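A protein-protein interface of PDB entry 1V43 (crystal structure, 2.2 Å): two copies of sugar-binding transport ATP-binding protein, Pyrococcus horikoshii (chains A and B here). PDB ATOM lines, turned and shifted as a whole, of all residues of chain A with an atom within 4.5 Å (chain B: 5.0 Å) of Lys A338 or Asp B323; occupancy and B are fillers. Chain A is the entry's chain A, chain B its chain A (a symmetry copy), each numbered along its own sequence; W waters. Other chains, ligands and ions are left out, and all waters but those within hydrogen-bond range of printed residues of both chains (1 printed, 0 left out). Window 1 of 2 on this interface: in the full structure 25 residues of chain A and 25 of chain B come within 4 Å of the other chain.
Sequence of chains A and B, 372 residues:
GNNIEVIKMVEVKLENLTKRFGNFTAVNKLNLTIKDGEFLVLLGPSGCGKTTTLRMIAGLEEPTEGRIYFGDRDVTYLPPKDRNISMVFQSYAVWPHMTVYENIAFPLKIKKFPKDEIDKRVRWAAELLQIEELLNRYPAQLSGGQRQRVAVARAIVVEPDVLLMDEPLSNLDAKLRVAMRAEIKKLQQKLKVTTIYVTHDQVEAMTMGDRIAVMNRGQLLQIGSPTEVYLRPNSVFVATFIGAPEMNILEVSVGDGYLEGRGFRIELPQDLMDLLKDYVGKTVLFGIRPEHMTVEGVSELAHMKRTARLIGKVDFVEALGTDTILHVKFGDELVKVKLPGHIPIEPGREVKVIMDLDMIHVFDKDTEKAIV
OE2 of Glu A291 lies close to OG1 of Thr B322, at 3.5 Å.
The side-chain amino group of Lys B338 lies within salt-bridge range of the side-chain carboxylate of Asp A323, at 2.6 Å.
NZ of Lys A338 sits at hydrogen-bond distance from OG1 of Thr B322 (3.0 Å).
The side-chain amino group (NZ) of Lys A338 lies within salt-bridge range of the side-chain carboxylate (OD2) of Asp B323 (2.6 Å).
N of Lys A338 lies within hydrogen-bond range of O of Pro A290, 3.0 Å away.
The backbone carbonyl oxygen (O) of Thr B322 is in hydrogen-bond range of the backbone NH (N) of Gly B341 (3.1 Å).
Among the printed residues, merely in contact across the chains: Pro A340 with Pro B340 (3.9 Å).
Printed residues of chain B within 4 Å of Lys A338: Thr B322 (3.0 Å) and Asp B323 (2.6 Å).
Asp B323 touches one residue of chain A.
Of the printed residues of chain B, Pro A340 touches Pro B340 (3.9 Å).
Of the printed residues of chain A, Thr B322 touches Glu A291 (3.4 Å) and Lys A338 (3.0 Å).
Gly B321 touches none of the printed residues of chain A.
Leu B339 touches none of the printed residues of chain A.
The nearest printed residue of chain B that does not touch Lys A338 is Lys B338 (5.4 Å).
The nearest residue of chain A that does not touch Asp B323 is Asp A323 (4.3 Å).
The nearest printed residue of chain B that does not touch Glu A291 is Gly B321 (4.5 Å).
Of the 12 printed residues of chain A, 4 touch a printed residue of chain B.
Hydrophobic or aromatic side chains of chain A that line the printed part of chain B: Pro A340.
Of the 12 printed residues of chain B, 4 touch a printed residue of chain A.
Hydrophobic or aromatic side chains of chain B that line the printed part of chain A: Pro B340.
Among the printed residues, 5 pairs touch across the chains.
Asp A323 touches Lys B338, and with the chains exchanged Lys A338 touches Asp B323.
Pro A340 touches its own counterpart, Pro B340.
Positions printed for both chains: 323, 324, 338, 339 and 340.
Of the 5 pairs that touch across the chains among the printed residues, 3 have their exchanged pair printed and touching as well.
Water W1 lies within hydrogen-bond range of the side-chain carboxylate of Glu A291 (2.6 Å), the backbone carbonyl oxygen of Pro A245 (3.0 Å) and the side-chain hydroxyl of Thr B322 (3.0 Å).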
ATOM      1  N   ALA A 244      -8.533 -32.084  29.169  1.00  0.00           N
ATOM      2  CA  ALA A 244      -8.200 -33.278  28.393  1.00  0.00           C
ATOM      3  C   ALA A 244      -9.144 -33.406  27.194  1.00  0.00           C
ATOM      4  O   ALA A 244     -10.352 -33.188  27.334  1.00  0.00           O
ATOM      5  CB  ALA A 244      -8.306 -34.537  29.300  1.00  0.00           C
ATOM      6  N   PRO A 245      -8.606 -33.701  25.991  1.00  0.00           N
ATOM      7  CA  PRO A 245      -7.192 -33.923  25.654  1.00  0.00           C
ATOM      8  C   PRO A 245      -6.335 -32.747  26.124  1.00  0.00           C
ATOM      9  O   PRO A 245      -6.780 -31.605  26.129  1.00  0.00           O
ATOM     10  CB  PRO A 245      -7.193 -33.988  24.131  1.00  0.00           C
ATOM     11  CG  PRO A 245      -8.576 -34.354  23.773  1.00  0.00           C
ATOM     12  CD  PRO A 245      -9.438 -33.683  24.773  1.00  0.00           C
ATOM     13  N   PRO A 290      -6.207 -28.215  22.182  1.00  0.00           N
ATOM     14  CA  PRO A 290      -6.972 -28.862  21.103  1.00  0.00           C
ATOM     15  C   PRO A 290      -8.279 -28.105  20.827  1.00  0.00           C
ATOM     16  O   PRO A 290      -8.663 -27.901  19.672  1.00  0.00           O
ATOM     17  CB  PRO A 290      -7.249 -30.260  21.657  1.00  0.00           C
ATOM     18  CG  PRO A 290      -6.012 -30.534  22.505  1.00  0.00           C
ATOM     19  CD  PRO A 290      -5.814 -29.196  23.217  1.00  0.00           C
ATOM     20  N   GLU A 291      -8.945 -27.685  21.902  1.00  0.00           N
ATOM     21  CA  GLU A 291     -10.208 -26.958  21.801  1.00  0.00           C
ATOM     22  C   GLU A 291     -10.035 -25.494  21.406  1.00  0.00           C
ATOM     23  O   GLU A 291     -11.029 -24.786  21.250  1.00  0.00           O
ATOM     24  CB  GLU A 291     -10.988 -27.024  23.123  1.00  0.00           C
ATOM     25  CG  GLU A 291     -10.327 -26.263  24.284  1.00  0.00           C
ATOM     26  CD  GLU A 291      -9.448 -27.150  25.165  1.00  0.00           C
ATOM     27  OE1 GLU A 291      -8.793 -28.070  24.640  1.00  0.00           O
ATOM     28  OE2 GLU A 291      -9.408 -26.917  26.390  1.00  0.00           O
ATOM     29  N   MET A 293      -8.338 -24.637  18.695  1.00  0.00           N
ATOM     30  CA  MET A 293      -7.994 -24.731  17.286  1.00  0.00           C
ATOM     31  C   MET A 293      -9.245 -25.232  16.597  1.00  0.00           C
ATOM     32  O   MET A 293     -10.188 -25.690  17.247  1.00  0.00           O
ATOM     33  CB  MET A 293      -6.867 -25.741  17.065  1.00  0.00           C
ATOM     34  CG  MET A 293      -5.528 -25.352  17.677  1.00  0.00           C
ATOM     35  SD  MET A 293      -4.386 -26.750  17.742  1.00  0.00           S
ATOM     36  CE  MET A 293      -3.954 -26.798  16.203  1.00  0.00           C
ATOM     37  N   ASP A 323     -17.956 -35.466  20.472  1.00  0.00           N
ATOM     38  CA  ASP A 323     -16.817 -34.641  20.053  1.00  0.00           C
ATOM     39  C   ASP A 323     -16.029 -35.459  19.039  1.00  0.00           C
ATOM     40  O   ASP A 323     -16.147 -36.681  19.002  1.00  0.00           O
ATOM     41  CB  ASP A 323     -15.887 -34.328  21.234  1.00  0.00           C
ATOM     42  CG  ASP A 323     -16.485 -33.343  22.192  1.00  0.00           C
ATOM     43  OD1 ASP A 323     -16.715 -32.186  21.775  1.00  0.00           O
ATOM     44  OD2 ASP A 323     -16.733 -33.724  23.355  1.00  0.00           O
ATOM     45  N   THR A 324     -15.223 -34.790  18.228  1.00  0.00           N
ATOM     46  CA  THR A 324     -14.407 -35.474  17.234  1.00  0.00           C
ATOM     47  C   THR A 324     -12.985 -34.973  17.407  1.00  0.00           C
ATOM     48  O   THR A 324     -12.711 -33.806  17.129  1.00  0.00           O
ATOM     49  CB  THR A 324     -14.877 -35.149  15.792  1.00  0.00           C
ATOM     50  OG1 THR A 324     -16.118 -35.809  15.531  1.00  0.00           O
ATOM     51  CG2 THR A 324     -13.837 -35.587  14.773  1.00  0.00           C
ATOM     52  N   LYS A 336      -3.303 -32.470  18.598  1.00  0.00           N
ATOM     53  CA  LYS A 336      -4.710 -32.866  18.620  1.00  0.00           C
ATOM     54  C   LYS A 336      -5.592 -31.653  18.479  1.00  0.00           C
ATOM     55  O   LYS A 336      -5.323 -30.617  19.074  1.00  0.00           O
ATOM     56  CB  LYS A 336      -5.068 -33.561  19.934  1.00  0.00           C
ATOM     57  CG  LYS A 336      -4.368 -34.879  20.165  1.00  0.00           C
ATOM     58  CD  LYS A 336      -4.750 -35.419  21.522  1.00  0.00           C
ATOM     59  CE  LYS A 336      -4.040 -36.710  21.841  1.00  0.00           C
ATOM     60  NZ  LYS A 336      -4.498 -37.230  23.157  1.00  0.00           N
ATOM     61  N   VAL A 337      -6.653 -31.797  17.694  1.00  0.00           N
ATOM     62  CA  VAL A 337      -7.618 -30.734  17.477  1.00  0.00           C
ATOM     63  C   VAL A 337      -8.987 -31.274  17.897  1.00  0.00           C
ATOM     64  O   VAL A 337      -9.426 -32.332  17.433  1.00  0.00           O
ATOM     65  CB  VAL A 337      -7.662 -30.308  15.999  1.00  0.00           C
ATOM     66  CG1 VAL A 337      -8.800 -29.321  15.774  1.00  0.00           C
ATOM     67  CG2 VAL A 337      -6.328 -29.671  15.603  1.00  0.00           C
ATOM     68  N   LYS A 338      -9.662 -30.552  18.782  1.00  0.00           N
ATOM     69  CA  LYS A 338     -10.958 -31.003  19.253  1.00  0.00           C
ATOM     70  C   LYS A 338     -12.113 -30.263  18.598  1.00  0.00           C
ATOM     71  O   LYS A 338     -12.242 -29.054  18.743  1.00  0.00           O
ATOM     72  CB  LYS A 338     -11.039 -30.851  20.772  1.00  0.00           C
ATOM     73  CG  LYS A 338     -12.363 -31.286  21.360  1.00  0.00           C
ATOM     74  CD  LYS A 338     -12.351 -31.122  22.867  1.00  0.00           C
ATOM     75  CE  LYS A 338     -13.700 -31.468  23.470  1.00  0.00           C
ATOM     76  NZ  LYS A 338     -13.669 -31.419  24.951  1.00  0.00           N
ATOM     77  N   LEU A 339     -12.952 -31.001  17.878  1.00  0.00           N
ATOM     78  CA  LEU A 339     -14.103 -30.418  17.209  1.00  0.00           C
ATOM     79  C   LEU A 339     -15.399 -30.916  17.845  1.00  0.00           C
ATOM     80  O   LEU A 339     -15.535 -32.101  18.143  1.00  0.00           O
ATOM     81  CB  LEU A 339     -14.111 -30.810  15.738  1.00  0.00           C
ATOM     82  CG  LEU A 339     -12.867 -30.487  14.915  1.00  0.00           C
ATOM     83  CD1 LEU A 339     -13.005 -31.133  13.541  1.00  0.00           C
ATOM     84  CD2 LEU A 339     -12.699 -28.971  14.802  1.00  0.00           C
ATOM     85  N   PRO A 340     -16.367 -30.012  18.066  1.00  0.00           N
ATOM     86  CA  PRO A 340     -17.654 -30.393  18.666  1.00  0.00           C
ATOM     87  C   PRO A 340     -18.436 -31.277  17.701  1.00  0.00           C
ATOM     88  O   PRO A 340     -18.291 -31.147  16.486  1.00  0.00           O
ATOM     89  CB  PRO A 340     -18.355 -29.049  18.886  1.00  0.00           C
ATOM     90  CG  PRO A 340     -17.191 -28.075  19.048  1.00  0.00           C
ATOM     91  CD  PRO A 340     -16.236 -28.546  17.970  1.00  0.00           C
ATOM     92  N   GLU B 318     -20.949 -27.120  35.300  1.00  0.00           N
ATOM     93  CA  GLU B 318     -19.678 -27.816  35.308  1.00  0.00           C
ATOM     94  C   GLU B 318     -18.857 -26.997  34.295  1.00  0.00           C
ATOM     95  O   GLU B 318     -18.948 -27.235  33.095  1.00  0.00           O
ATOM     96  CB  GLU B 318     -19.816 -29.253  34.784  1.00  0.00           C
ATOM     97  CG  GLU B 318     -20.731 -30.180  35.559  1.00  0.00           C
ATOM     98  CD  GLU B 318     -20.800 -31.567  34.917  1.00  0.00           C
ATOM     99  OE1 GLU B 318     -19.734 -32.169  34.697  1.00  0.00           O
ATOM    100  OE2 GLU B 318     -21.908 -32.062  34.626  1.00  0.00           O
ATOM    101  N   ALA B 319     -18.093 -26.020  34.769  1.00  0.00           N
ATOM    102  CA  ALA B 319     -17.263 -25.191  33.882  1.00  0.00           C
ATOM    103  C   ALA B 319     -15.910 -25.887  33.792  1.00  0.00           C
ATOM    104  O   ALA B 319     -15.004 -25.596  34.573  1.00  0.00           O
ATOM    105  CB  ALA B 319     -17.100 -23.792  34.475  1.00  0.00           C
ATOM    106  N   LEU B 320     -15.772 -26.799  32.836  1.00  0.00           N
ATOM    107  CA  LEU B 320     -14.549 -27.584  32.725  1.00  0.00           C
ATOM    108  C   LEU B 320     -13.465 -27.002  31.839  1.00  0.00           C
ATOM    109  O   LEU B 320     -12.464 -27.680  31.557  1.00  0.00           O
ATOM    110  CB  LEU B 320     -14.899 -29.004  32.255  1.00  0.00           C
ATOM    111  CG  LEU B 320     -16.130 -29.587  32.960  1.00  0.00           C
ATOM    112  CD1 LEU B 320     -16.505 -30.937  32.374  1.00  0.00           C
ATOM    113  CD2 LEU B 320     -15.833 -29.708  34.444  1.00  0.00           C
ATOM    114  N   GLY B 321     -13.657 -25.756  31.409  1.00  0.00           N
ATOM    115  CA  GLY B 321     -12.681 -25.097  30.556  1.00  0.00           C
ATOM    116  C   GLY B 321     -12.784 -25.560  29.111  1.00  0.00           C
ATOM    117  O   GLY B 321     -13.035 -24.757  28.209  1.00  0.00           O
ATOM    118  N   THR B 322     -12.598 -26.859  28.884  1.00  0.00           N
ATOM    119  CA  THR B 322     -12.682 -27.420  27.541  1.00  0.00           C
ATOM    120  C   THR B 322     -14.148 -27.496  27.061  1.00  0.00           C
ATOM    121  O   THR B 322     -14.424 -27.406  25.870  1.00  0.00           O
ATOM    122  CB  THR B 322     -12.007 -28.822  27.508  1.00  0.00           C
ATOM    123  OG1 THR B 322     -11.939 -29.295  26.153  1.00  0.00           O
ATOM    124  CG2 THR B 322     -12.784 -29.812  28.378  1.00  0.00           C
ATOM    125  N   ASP B 323     -15.072 -27.641  28.010  1.00  0.00           N
ATOM    126  CA  ASP B 323     -16.516 -27.707  27.758  1.00  0.00           C
ATOM    127  C   ASP B 323     -17.205 -27.134  28.988  1.00  0.00           C
ATOM    128  O   ASP B 323     -16.614 -27.087  30.065  1.00  0.00           O
ATOM    129  CB  ASP B 323     -16.988 -29.157  27.583  1.00  0.00           C
ATOM    130  CG  ASP B 323     -16.546 -29.753  26.281  1.00  0.00           C
ATOM    131  OD1 ASP B 323     -16.987 -29.245  25.225  1.00  0.00           O
ATOM    132  OD2 ASP B 323     -15.757 -30.720  26.309  1.00  0.00           O
ATOM    133  N   THR B 324     -18.451 -26.710  28.833  1.00  0.00           N
ATOM    134  CA  THR B 324     -19.212 -26.163  29.949  1.00  0.00           C
ATOM    135  C   THR B 324     -20.541 -26.894  29.979  1.00  0.00           C
ATOM    136  O   THR B 324     -21.354 -26.721  29.072  1.00  0.00           O
ATOM    137  CB  THR B 324     -19.482 -24.647  29.763  1.00  0.00           C
ATOM    138  OG1 THR B 324     -18.269 -23.915  29.960  1.00  0.00           O
ATOM    139  CG2 THR B 324     -20.540 -24.163  30.740  1.00  0.00           C
ATOM    140  N   ILE B 325     -20.761 -27.718  30.999  1.00  0.00           N
ATOM    141  CA  ILE B 325     -22.016 -28.461  31.088  1.00  0.00           C
ATOM    142  C   ILE B 325     -23.029 -27.824  32.031  1.00  0.00           C
ATOM    143  O   ILE B 325     -22.797 -27.704  33.239  1.00  0.00           O
ATOM    144  CB  ILE B 325     -21.783 -29.906  31.535  1.00  0.00           C
ATOM    145  CG1 ILE B 325     -20.740 -30.545  30.628  1.00  0.00           C
ATOM    146  CG2 ILE B 325     -23.109 -30.702  31.452  1.00  0.00           C
ATOM    147  CD1 ILE B 325     -20.397 -31.958  31.004  1.00  0.00           C
ATOM    148  N   LYS B 338     -24.637 -29.392  26.903  1.00  0.00           N
ATOM    149  CA  LYS B 338     -23.197 -29.298  26.748  1.00  0.00           C
ATOM    150  C   LYS B 338     -22.781 -28.202  25.780  1.00  0.00           C
ATOM    151  O   LYS B 338     -23.121 -28.246  24.604  1.00  0.00           O
ATOM    152  CB  LYS B 338     -22.638 -30.642  26.283  1.00  0.00           C
ATOM    153  CG  LYS B 338     -21.138 -30.641  26.079  1.00  0.00           C
ATOM    154  CD  LYS B 338     -20.665 -32.013  25.640  1.00  0.00           C
ATOM    155  CE  LYS B 338     -19.178 -32.014  25.343  1.00  0.00           C
ATOM    156  NZ  LYS B 338     -18.682 -33.373  25.020  1.00  0.00           N
ATOM    157  N   LEU B 339     -22.040 -27.221  26.285  1.00  0.00           N
ATOM    158  CA  LEU B 339     -21.566 -26.119  25.464  1.00  0.00           C
ATOM    159  C   LEU B 339     -20.046 -26.176  25.319  1.00  0.00           C
ATOM    160  O   LEU B 339     -19.334 -26.426  26.289  1.00  0.00           O
ATOM    161  CB  LEU B 339     -21.935 -24.789  26.106  1.00  0.00           C
ATOM    162  CG  LEU B 339     -23.407 -24.546  26.427  1.00  0.00           C
ATOM    163  CD1 LEU B 339     -23.528 -23.257  27.233  1.00  0.00           C
ATOM    164  CD2 LEU B 339     -24.216 -24.468  25.131  1.00  0.00           C
ATOM    165  N   PRO B 340     -19.533 -25.951  24.099  1.00  0.00           N
ATOM    166  CA  PRO B 340     -18.083 -25.975  23.857  1.00  0.00           C
ATOM    167  C   PRO B 340     -17.418 -24.799  24.564  1.00  0.00           C
ATOM    168  O   PRO B 340     -18.038 -23.749  24.737  1.00  0.00           O
ATOM    169  CB  PRO B 340     -17.974 -25.846  22.335  1.00  0.00           C
ATOM    170  CG  PRO B 340     -19.289 -26.447  21.843  1.00  0.00           C
ATOM    171  CD  PRO B 340     -20.284 -25.875  22.832  1.00  0.00           C
ATOM    172  N   GLY B 341     -16.169 -24.976  24.985  1.00  0.00           N
ATOM    173  CA  GLY B 341     -15.460 -23.890  25.640  1.00  0.00           C
ATOM    174  C   GLY B 341     -15.851 -23.625  27.081  1.00  0.00           C
ATOM    175  O   GLY B 341     -16.628 -24.377  27.676  1.00  0.00           O
HETATM  176  O   HOH W   1      -9.399 -30.544  25.140  1.00  0.00           O
